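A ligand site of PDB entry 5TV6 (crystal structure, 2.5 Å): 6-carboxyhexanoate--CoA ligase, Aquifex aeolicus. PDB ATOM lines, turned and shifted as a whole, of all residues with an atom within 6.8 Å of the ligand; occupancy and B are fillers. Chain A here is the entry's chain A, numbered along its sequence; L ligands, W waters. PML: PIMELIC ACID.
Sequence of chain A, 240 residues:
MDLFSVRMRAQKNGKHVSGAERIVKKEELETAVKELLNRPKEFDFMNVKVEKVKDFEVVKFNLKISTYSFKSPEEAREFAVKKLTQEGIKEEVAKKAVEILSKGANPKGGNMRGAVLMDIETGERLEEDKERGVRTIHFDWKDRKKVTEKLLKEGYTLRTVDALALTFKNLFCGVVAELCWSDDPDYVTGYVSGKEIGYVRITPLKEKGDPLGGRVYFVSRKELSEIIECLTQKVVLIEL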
ATOM      1  N   TYR A 156      20.694  21.906 -23.701  1.00  0.00           N
ATOM      2  CA  TYR A 156      19.787  21.077 -22.926  1.00  0.00           C
ATOM      3  C   TYR A 156      20.256  19.616 -22.926  1.00  0.00           C
ATOM      4  O   TYR A 156      21.195  19.236 -23.615  1.00  0.00           O
ATOM      5  CB  TYR A 156      18.378  21.204 -23.484  1.00  0.00           C
ATOM      6  CG  TYR A 156      17.912  22.621 -23.450  1.00  0.00           C
ATOM      7  CD1 TYR A 156      17.748  23.279 -22.234  1.00  0.00           C
ATOM      8  CD2 TYR A 156      17.647  23.329 -24.629  1.00  0.00           C
ATOM      9  CE1 TYR A 156      17.325  24.603 -22.172  1.00  0.00           C
ATOM     10  CE2 TYR A 156      17.214  24.661 -24.579  1.00  0.00           C
ATOM     11  CZ  TYR A 156      17.058  25.278 -23.347  1.00  0.00           C
ATOM     12  OH  TYR A 156      16.639  26.591 -23.254  1.00  0.00           O
ATOM     13  N   THR A 157      19.581  18.793 -22.123  1.00  0.00           N
ATOM     14  CA  THR A 157      19.910  17.382 -22.028  1.00  0.00           C
ATOM     15  C   THR A 157      18.892  16.525 -22.807  1.00  0.00           C
ATOM     16  O   THR A 157      17.906  17.027 -23.370  1.00  0.00           O
ATOM     17  CB  THR A 157      19.968  16.929 -20.567  1.00  0.00           C
ATOM     18  OG1 THR A 157      18.661  16.995 -19.992  1.00  0.00           O
ATOM     19  CG2 THR A 157      20.901  17.817 -19.766  1.00  0.00           C
ATOM     20  N   ARG A 159      17.041  14.432 -21.284  1.00  0.00           N
ATOM     21  CA  ARG A 159      15.849  14.434 -20.443  1.00  0.00           C
ATOM     22  C   ARG A 159      14.952  15.618 -20.760  1.00  0.00           C
ATOM     23  O   ARG A 159      13.720  15.485 -20.708  1.00  0.00           O
ATOM     24  CB  ARG A 159      16.229  14.435 -18.962  1.00  0.00           C
ATOM     25  CG  ARG A 159      16.726  13.127 -18.469  1.00  0.00           C
ATOM     26  CD  ARG A 159      17.075  13.235 -17.000  1.00  0.00           C
ATOM     27  NE  ARG A 159      17.802  12.064 -16.530  1.00  0.00           N
ATOM     28  CZ  ARG A 159      17.249  11.079 -15.825  1.00  0.00           C
ATOM     29  NH1 ARG A 159      15.957  11.129 -15.525  1.00  0.00           N
ATOM     30  NH2 ARG A 159      17.994  10.049 -15.441  1.00  0.00           N
ATOM     31  N   THR A 160      15.534  16.784 -21.062  1.00  0.00           N
ATOM     32  CA  THR A 160      14.742  17.911 -21.528  1.00  0.00           C
ATOM     33  C   THR A 160      13.962  17.527 -22.785  1.00  0.00           C
ATOM     34  O   THR A 160      12.765  17.812 -22.900  1.00  0.00           O
ATOM     35  CB  THR A 160      15.624  19.120 -21.838  1.00  0.00           C
ATOM     36  OG1 THR A 160      16.483  19.415 -20.722  1.00  0.00           O
ATOM     37  CG2 THR A 160      14.776  20.343 -22.144  1.00  0.00           C
ATOM     38  N   VAL A 161      14.653  16.898 -23.731  1.00  0.00           N
ATOM     39  CA  VAL A 161      14.008  16.552 -24.994  1.00  0.00           C
ATOM     40  C   VAL A 161      12.774  15.721 -24.731  1.00  0.00           C
ATOM     41  O   VAL A 161      11.701  15.967 -25.282  1.00  0.00           O
ATOM     42  CB  VAL A 161      15.002  15.804 -25.903  1.00  0.00           C
ATOM     43  CG1 VAL A 161      14.341  15.467 -27.222  1.00  0.00           C
ATOM     44  CG2 VAL A 161      16.268  16.630 -26.094  1.00  0.00           C
ATOM     45  N   ALA A 163      11.141  15.400 -21.717  1.00  0.00           N
ATOM     46  CA  ALA A 163      10.190  16.092 -20.848  1.00  0.00           C
ATOM     47  C   ALA A 163       9.406  17.148 -21.610  1.00  0.00           C
ATOM     48  O   ALA A 163       8.210  17.352 -21.348  1.00  0.00           O
ATOM     49  CB  ALA A 163      10.909  16.704 -19.663  1.00  0.00           C
ATOM     50  N   LEU A 164      10.056  17.835 -22.562  1.00  0.00           N
ATOM     51  CA  LEU A 164       9.378  18.846 -23.364  1.00  0.00           C
ATOM     52  C   LEU A 164       8.209  18.254 -24.119  1.00  0.00           C
ATOM     53  O   LEU A 164       7.079  18.750 -24.027  1.00  0.00           O
ATOM     54  CB  LEU A 164      10.346  19.490 -24.356  1.00  0.00           C
ATOM     55  CG  LEU A 164      11.011  20.792 -23.962  1.00  0.00           C
ATOM     56  CD1 LEU A 164      11.903  21.239 -25.118  1.00  0.00           C
ATOM     57  CD2 LEU A 164       9.942  21.832 -23.604  1.00  0.00           C
ATOM     58  N   CYS A 180       7.048  18.880 -11.764  1.00  0.00           N
ATOM     59  CA  CYS A 180       7.805  17.671 -12.054  1.00  0.00           C
ATOM     60  C   CYS A 180       9.256  17.835 -11.633  1.00  0.00           C
ATOM     61  O   CYS A 180       9.882  18.859 -11.958  1.00  0.00           O
ATOM     62  CB  CYS A 180       7.744  17.338 -13.564  1.00  0.00           C
ATOM     63  SG  CYS A 180       8.948  16.106 -14.117  1.00  0.00           S
ATOM     64  N   TRP A 181       9.796  16.846 -10.931  1.00  0.00           N
ATOM     65  CA  TRP A 181      11.239  16.646 -10.928  1.00  0.00           C
ATOM     66  C   TRP A 181      11.524  15.155 -10.977  1.00  0.00           C
ATOM     67  O   TRP A 181      10.617  14.325 -10.881  1.00  0.00           O
ATOM     68  CB  TRP A 181      11.932  17.333  -9.737  1.00  0.00           C
ATOM     69  CG  TRP A 181      11.574  16.929  -8.339  1.00  0.00           C
ATOM     70  CD1 TRP A 181      12.100  15.891  -7.619  1.00  0.00           C
ATOM     71  CD2 TRP A 181      10.663  17.612  -7.448  1.00  0.00           C
ATOM     72  NE1 TRP A 181      11.555  15.867  -6.356  1.00  0.00           N
ATOM     73  CE2 TRP A 181      10.678  16.908  -6.227  1.00  0.00           C
ATOM     74  CE3 TRP A 181       9.842  18.736  -7.584  1.00  0.00           C
ATOM     75  CZ2 TRP A 181       9.886  17.288  -5.144  1.00  0.00           C
ATOM     76  CZ3 TRP A 181       9.057  19.109  -6.511  1.00  0.00           C
ATOM     77  CH2 TRP A 181       9.090  18.390  -5.297  1.00  0.00           C
ATOM     78  N   SER A 182      12.785  14.823 -11.212  1.00  0.00           N
ATOM     79  CA  SER A 182      13.134  13.449 -11.517  1.00  0.00           C
ATOM     80  C   SER A 182      13.212  12.623 -10.235  1.00  0.00           C
ATOM     81  O   SER A 182      13.426  13.148  -9.143  1.00  0.00           O
ATOM     82  CB  SER A 182      14.471  13.395 -12.250  1.00  0.00           C
ATOM     83  OG  SER A 182      14.739  12.115 -12.785  1.00  0.00           O
ATOM     84  N   ASP A 183      13.051  11.311 -10.385  1.00  0.00           N
ATOM     85  CA  ASP A 183      13.345  10.436  -9.259  1.00  0.00           C
ATOM     86  C   ASP A 183      14.752   9.886  -9.299  1.00  0.00           C
ATOM     87  O   ASP A 183      15.214   9.346  -8.295  1.00  0.00           O
ATOM     88  CB  ASP A 183      12.325   9.300  -9.157  1.00  0.00           C
ATOM     89  CG  ASP A 183      11.938   8.721 -10.491  1.00  0.00           C
ATOM     90  OD1 ASP A 183      12.831   8.176 -11.182  1.00  0.00           O
ATOM     91  OD2 ASP A 183      10.724   8.772 -10.813  1.00  0.00           O
ATOM     92  N   ASP A 184      15.453  10.009 -10.434  1.00  0.00           N
ATOM     93  CA  ASP A 184      16.883   9.754 -10.466  1.00  0.00           C
ATOM     94  C   ASP A 184      17.568  10.586  -9.388  1.00  0.00           C
ATOM     95  O   ASP A 184      17.375  11.812  -9.349  1.00  0.00           O
ATOM     96  CB  ASP A 184      17.446  10.091 -11.846  1.00  0.00           C
ATOM     97  CG  ASP A 184      18.935   9.812 -11.992  1.00  0.00           C
ATOM     98  OD1 ASP A 184      19.717  10.018 -11.043  1.00  0.00           O
ATOM     99  OD2 ASP A 184      19.345   9.403 -13.099  1.00  0.00           O
ATOM    100  N   TYR A 187      19.942  13.593 -10.694  1.00  0.00           N
ATOM    101  CA  TYR A 187      19.440  14.593 -11.636  1.00  0.00           C
ATOM    102  C   TYR A 187      18.424  15.463 -10.902  1.00  0.00           C
ATOM    103  O   TYR A 187      17.292  15.053 -10.658  1.00  0.00           O
ATOM    104  CB  TYR A 187      18.825  13.935 -12.851  1.00  0.00           C
ATOM    105  CG  TYR A 187      18.573  14.860 -14.019  1.00  0.00           C
ATOM    106  CD1 TYR A 187      17.422  15.647 -14.071  1.00  0.00           C
ATOM    107  CD2 TYR A 187      19.470  14.951 -15.080  1.00  0.00           C
ATOM    108  CE1 TYR A 187      17.182  16.482 -15.125  1.00  0.00           C
ATOM    109  CE2 TYR A 187      19.241  15.791 -16.139  1.00  0.00           C
ATOM    110  CZ  TYR A 187      18.097  16.556 -16.162  1.00  0.00           C
ATOM    111  OH  TYR A 187      17.856  17.403 -17.224  1.00  0.00           O
ATOM    112  N   THR A 189      17.374  18.704 -11.684  1.00  0.00           N
ATOM    113  CA  THR A 189      16.670  19.733 -12.427  1.00  0.00           C
ATOM    114  C   THR A 189      15.256  19.231 -12.709  1.00  0.00           C
ATOM    115  O   THR A 189      15.073  18.092 -13.141  1.00  0.00           O
ATOM    116  CB  THR A 189      17.375  20.085 -13.752  1.00  0.00           C
ATOM    117  OG1 THR A 189      18.697  20.600 -13.507  1.00  0.00           O
ATOM    118  CG2 THR A 189      16.617  21.150 -14.505  1.00  0.00           C
ATOM    119  N   GLY A 190      14.282  20.080 -12.474  1.00  0.00           N
ATOM    120  CA  GLY A 190      12.912  19.712 -12.782  1.00  0.00           C
ATOM    121  C   GLY A 190      12.246  20.859 -13.492  1.00  0.00           C
ATOM    122  O   GLY A 190      12.929  21.672 -14.125  1.00  0.00           O
ATOM    123  N   TYR A 191      10.925  20.957 -13.403  1.00  0.00           N
ATOM    124  CA  TYR A 191      10.308  22.068 -14.095  1.00  0.00           C
ATOM    125  C   TYR A 191       8.895  22.304 -13.595  1.00  0.00           C
ATOM    126  O   TYR A 191       8.292  21.454 -12.935  1.00  0.00           O
ATOM    127  CB  TYR A 191      10.303  21.872 -15.605  1.00  0.00           C
ATOM    128  CG  TYR A 191       9.543  20.660 -16.096  1.00  0.00           C
ATOM    129  CD1 TYR A 191       8.193  20.743 -16.347  1.00  0.00           C
ATOM    130  CD2 TYR A 191      10.195  19.453 -16.344  1.00  0.00           C
ATOM    131  CE1 TYR A 191       7.496  19.647 -16.809  1.00  0.00           C
ATOM    132  CE2 TYR A 191       9.500  18.348 -16.807  1.00  0.00           C
ATOM    133  CZ  TYR A 191       8.147  18.459 -17.043  1.00  0.00           C
ATOM    134  OH  TYR A 191       7.418  17.406 -17.517  1.00  0.00           O
ATOM    135  N   TYR A 199       7.752  26.535 -20.413  1.00  0.00           N
ATOM    136  CA  TYR A 199       8.506  25.437 -19.805  1.00  0.00           C
ATOM    137  C   TYR A 199       9.603  26.059 -18.939  1.00  0.00           C
ATOM    138  O   TYR A 199      10.633  26.508 -19.461  1.00  0.00           O
ATOM    139  CB  TYR A 199       9.058  24.514 -20.900  1.00  0.00           C
ATOM    140  CG  TYR A 199       9.787  23.287 -20.386  1.00  0.00           C
ATOM    141  CD1 TYR A 199       9.085  22.219 -19.838  1.00  0.00           C
ATOM    142  CD2 TYR A 199      11.168  23.199 -20.466  1.00  0.00           C
ATOM    143  CE1 TYR A 199       9.762  21.094 -19.364  1.00  0.00           C
ATOM    144  CE2 TYR A 199      11.842  22.094 -20.000  1.00  0.00           C
ATOM    145  CZ  TYR A 199      11.135  21.046 -19.459  1.00  0.00           C
ATOM    146  OH  TYR A 199      11.823  19.968 -18.995  1.00  0.00           O
ATOM    147  N   ARG A 201      12.384  25.561 -16.471  1.00  0.00           N
ATOM    148  CA  ARG A 201      13.307  24.628 -15.835  1.00  0.00           C
ATOM    149  C   ARG A 201      13.854  25.258 -14.561  1.00  0.00           C
ATOM    150  O   ARG A 201      14.232  26.434 -14.551  1.00  0.00           O
ATOM    151  CB  ARG A 201      14.445  24.233 -16.786  1.00  0.00           C
ATOM    152  CG  ARG A 201      13.971  23.852 -18.184  1.00  0.00           C
ATOM    153  CD  ARG A 201      15.110  23.655 -19.225  1.00  0.00           C
ATOM    154  NE  ARG A 201      16.049  22.599 -18.861  1.00  0.00           N
ATOM    155  CZ  ARG A 201      17.326  22.792 -18.507  1.00  0.00           C
ATOM    156  NH1 ARG A 201      17.853  24.021 -18.496  1.00  0.00           N
ATOM    157  NH2 ARG A 201      18.089  21.741 -18.185  1.00  0.00           N
ATOM    158  N   ILE A 202      13.876  24.481 -13.477  1.00  0.00           N
ATOM    159  CA  ILE A 202      14.299  24.923 -12.147  1.00  0.00           C
ATOM    160  C   ILE A 202      15.298  23.909 -11.620  1.00  0.00           C
ATOM    161  O   ILE A 202      15.045  22.705 -11.672  1.00  0.00           O
ATOM    162  CB  ILE A 202      13.095  25.040 -11.193  1.00  0.00           C
ATOM    163  CG1 ILE A 202      12.026  25.931 -11.817  1.00  0.00           C
ATOM    164  CG2 ILE A 202      13.539  25.497  -9.811  1.00  0.00           C
ATOM    165  CD1 ILE A 202      10.751  25.919 -11.045  1.00  0.00           C
ATOM    166  N   GLY A 214       8.602  12.592  -9.416  1.00  0.00           N
ATOM    167  CA  GLY A 214       7.272  12.361  -9.930  1.00  0.00           C
ATOM    168  C   GLY A 214       6.686  13.584 -10.560  1.00  0.00           C
ATOM    169  O   GLY A 214       7.296  14.653 -10.575  1.00  0.00           O
ATOM    170  N   ARG A 215       5.491  13.436 -11.125  1.00  0.00           N
ATOM    171  CA  ARG A 215       4.783  14.540 -11.739  1.00  0.00           C
ATOM    172  C   ARG A 215       3.475  14.763 -10.998  1.00  0.00           C
ATOM    173  O   ARG A 215       2.983  13.876 -10.301  1.00  0.00           O
ATOM    174  CB  ARG A 215       4.511  14.280 -13.224  1.00  0.00           C
ATOM    175  CG  ARG A 215       5.722  14.501 -14.104  1.00  0.00           C
ATOM    176  CD  ARG A 215       5.501  14.051 -15.524  1.00  0.00           C
ATOM    177  NE  ARG A 215       6.591  13.183 -15.939  1.00  0.00           N
ATOM    178  CZ  ARG A 215       7.687  13.589 -16.575  1.00  0.00           C
ATOM    179  NH1 ARG A 215       7.836  14.860 -16.913  1.00  0.00           N
ATOM    180  NH2 ARG A 215       8.619  12.709 -16.881  1.00  0.00           N
HETATM  181  C1  PML L   1      12.391  13.169 -15.509  1.00  0.00           C
HETATM  182  O11 PML L   1      11.392  12.643 -14.940  1.00  0.00           O
HETATM  183  O12 PML L   1      13.495  12.538 -15.623  1.00  0.00           O
HETATM  184  C2  PML L   1      12.269  14.583 -16.061  1.00  0.00           C
HETATM  185  C3  PML L   1      13.429  15.435 -15.548  1.00  0.00           C
HETATM  186  C4  PML L   1      13.158  16.922 -15.655  1.00  0.00           C
HETATM  187  C5  PML L   1      13.632  17.479 -16.990  1.00  0.00           C
HETATM  188  C6  PML L   1      14.202  18.866 -16.747  1.00  0.00           C
HETATM  189  C7  PML L   1      15.043  19.350 -17.922  1.00  0.00           C
HETATM  190  O71 PML L   1      14.458  19.906 -18.875  1.00  0.00           O
HETATM  191  O72 PML L   1      16.298  19.190 -17.925  1.00  0.00           O
HETATM  192  O   HOH W   1      12.874  13.138 -18.994  1.00  0.00           O
HETATM  193  O   HOH W   2       9.539  12.361 -12.897  1.00  0.00           O
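An oxygen (O72) of the ligand lies within hydrogen-bond range of the side-chain hydroxyl of Tyr 187 (2.5 Å). OH of Tyr 199 sits at hydrogen-bond distance from O71 of the ligand (2.6 Å). The side-chain hydroxyl of Thr 160 sits at hydrogen-bond distance from an oxygen (O71) of the ligand (2.8 Å). O12 of the ligand is in salt-bridge range of NH1 of Arg 159, at 2.8 Å. OG of Ser 182 lies within hydrogen-bond range of O12 of the ligand, 3.1 Å away. NE of Arg 201 lies within salt-bridge range of O71 of the ligand (3.1 Å). An oxygen (O11) of the ligand lies within salt-bridge range of the guanidinium group of Arg 215 (3.4 Å).
Water W2 lies within hydrogen-bond range of O11 of the ligand (2.8 Å) and O of Trp 181 (3.0 Å). Water W1 lies within hydrogen-bond range of O of Arg 159 and O12 of the ligand.
Thr 157 touches the ligand. Ala 163 touches the ligand. O of Thr 189 touches C4 of the ligand, at 3.4 Å. Tyr 191 touches the ligand. Along chain A the residues within 4 Å of the ligand span positions 157 to 215.
OH of Tyr 187 lies within hydrogen-bond range of OG1 of Thr 157 (2.9 Å). OG1 of Thr 157 is in hydrogen-bond range of N of Thr 160 (3.3 Å). NH1 of Arg 159 is in hydrogen-bond range of OG of Ser 182 (3.2 Å). N of Arg 159 lies close to OG1 of Thr 157 (3.3 Å). OD2 of Asp 184 lies within salt-bridge range of NH2 of Arg 159. OG of Ser 182 sits at hydrogen-bond distance from N of Asp 184. The guanidinium group (NH1) of Arg 215 lies within hydrogen-bond range of the side-chain hydroxyl (OH) of Tyr 191. N of Tyr 191 is in hydrogen-bond range of O of Cys 180, at 2.8 Å.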
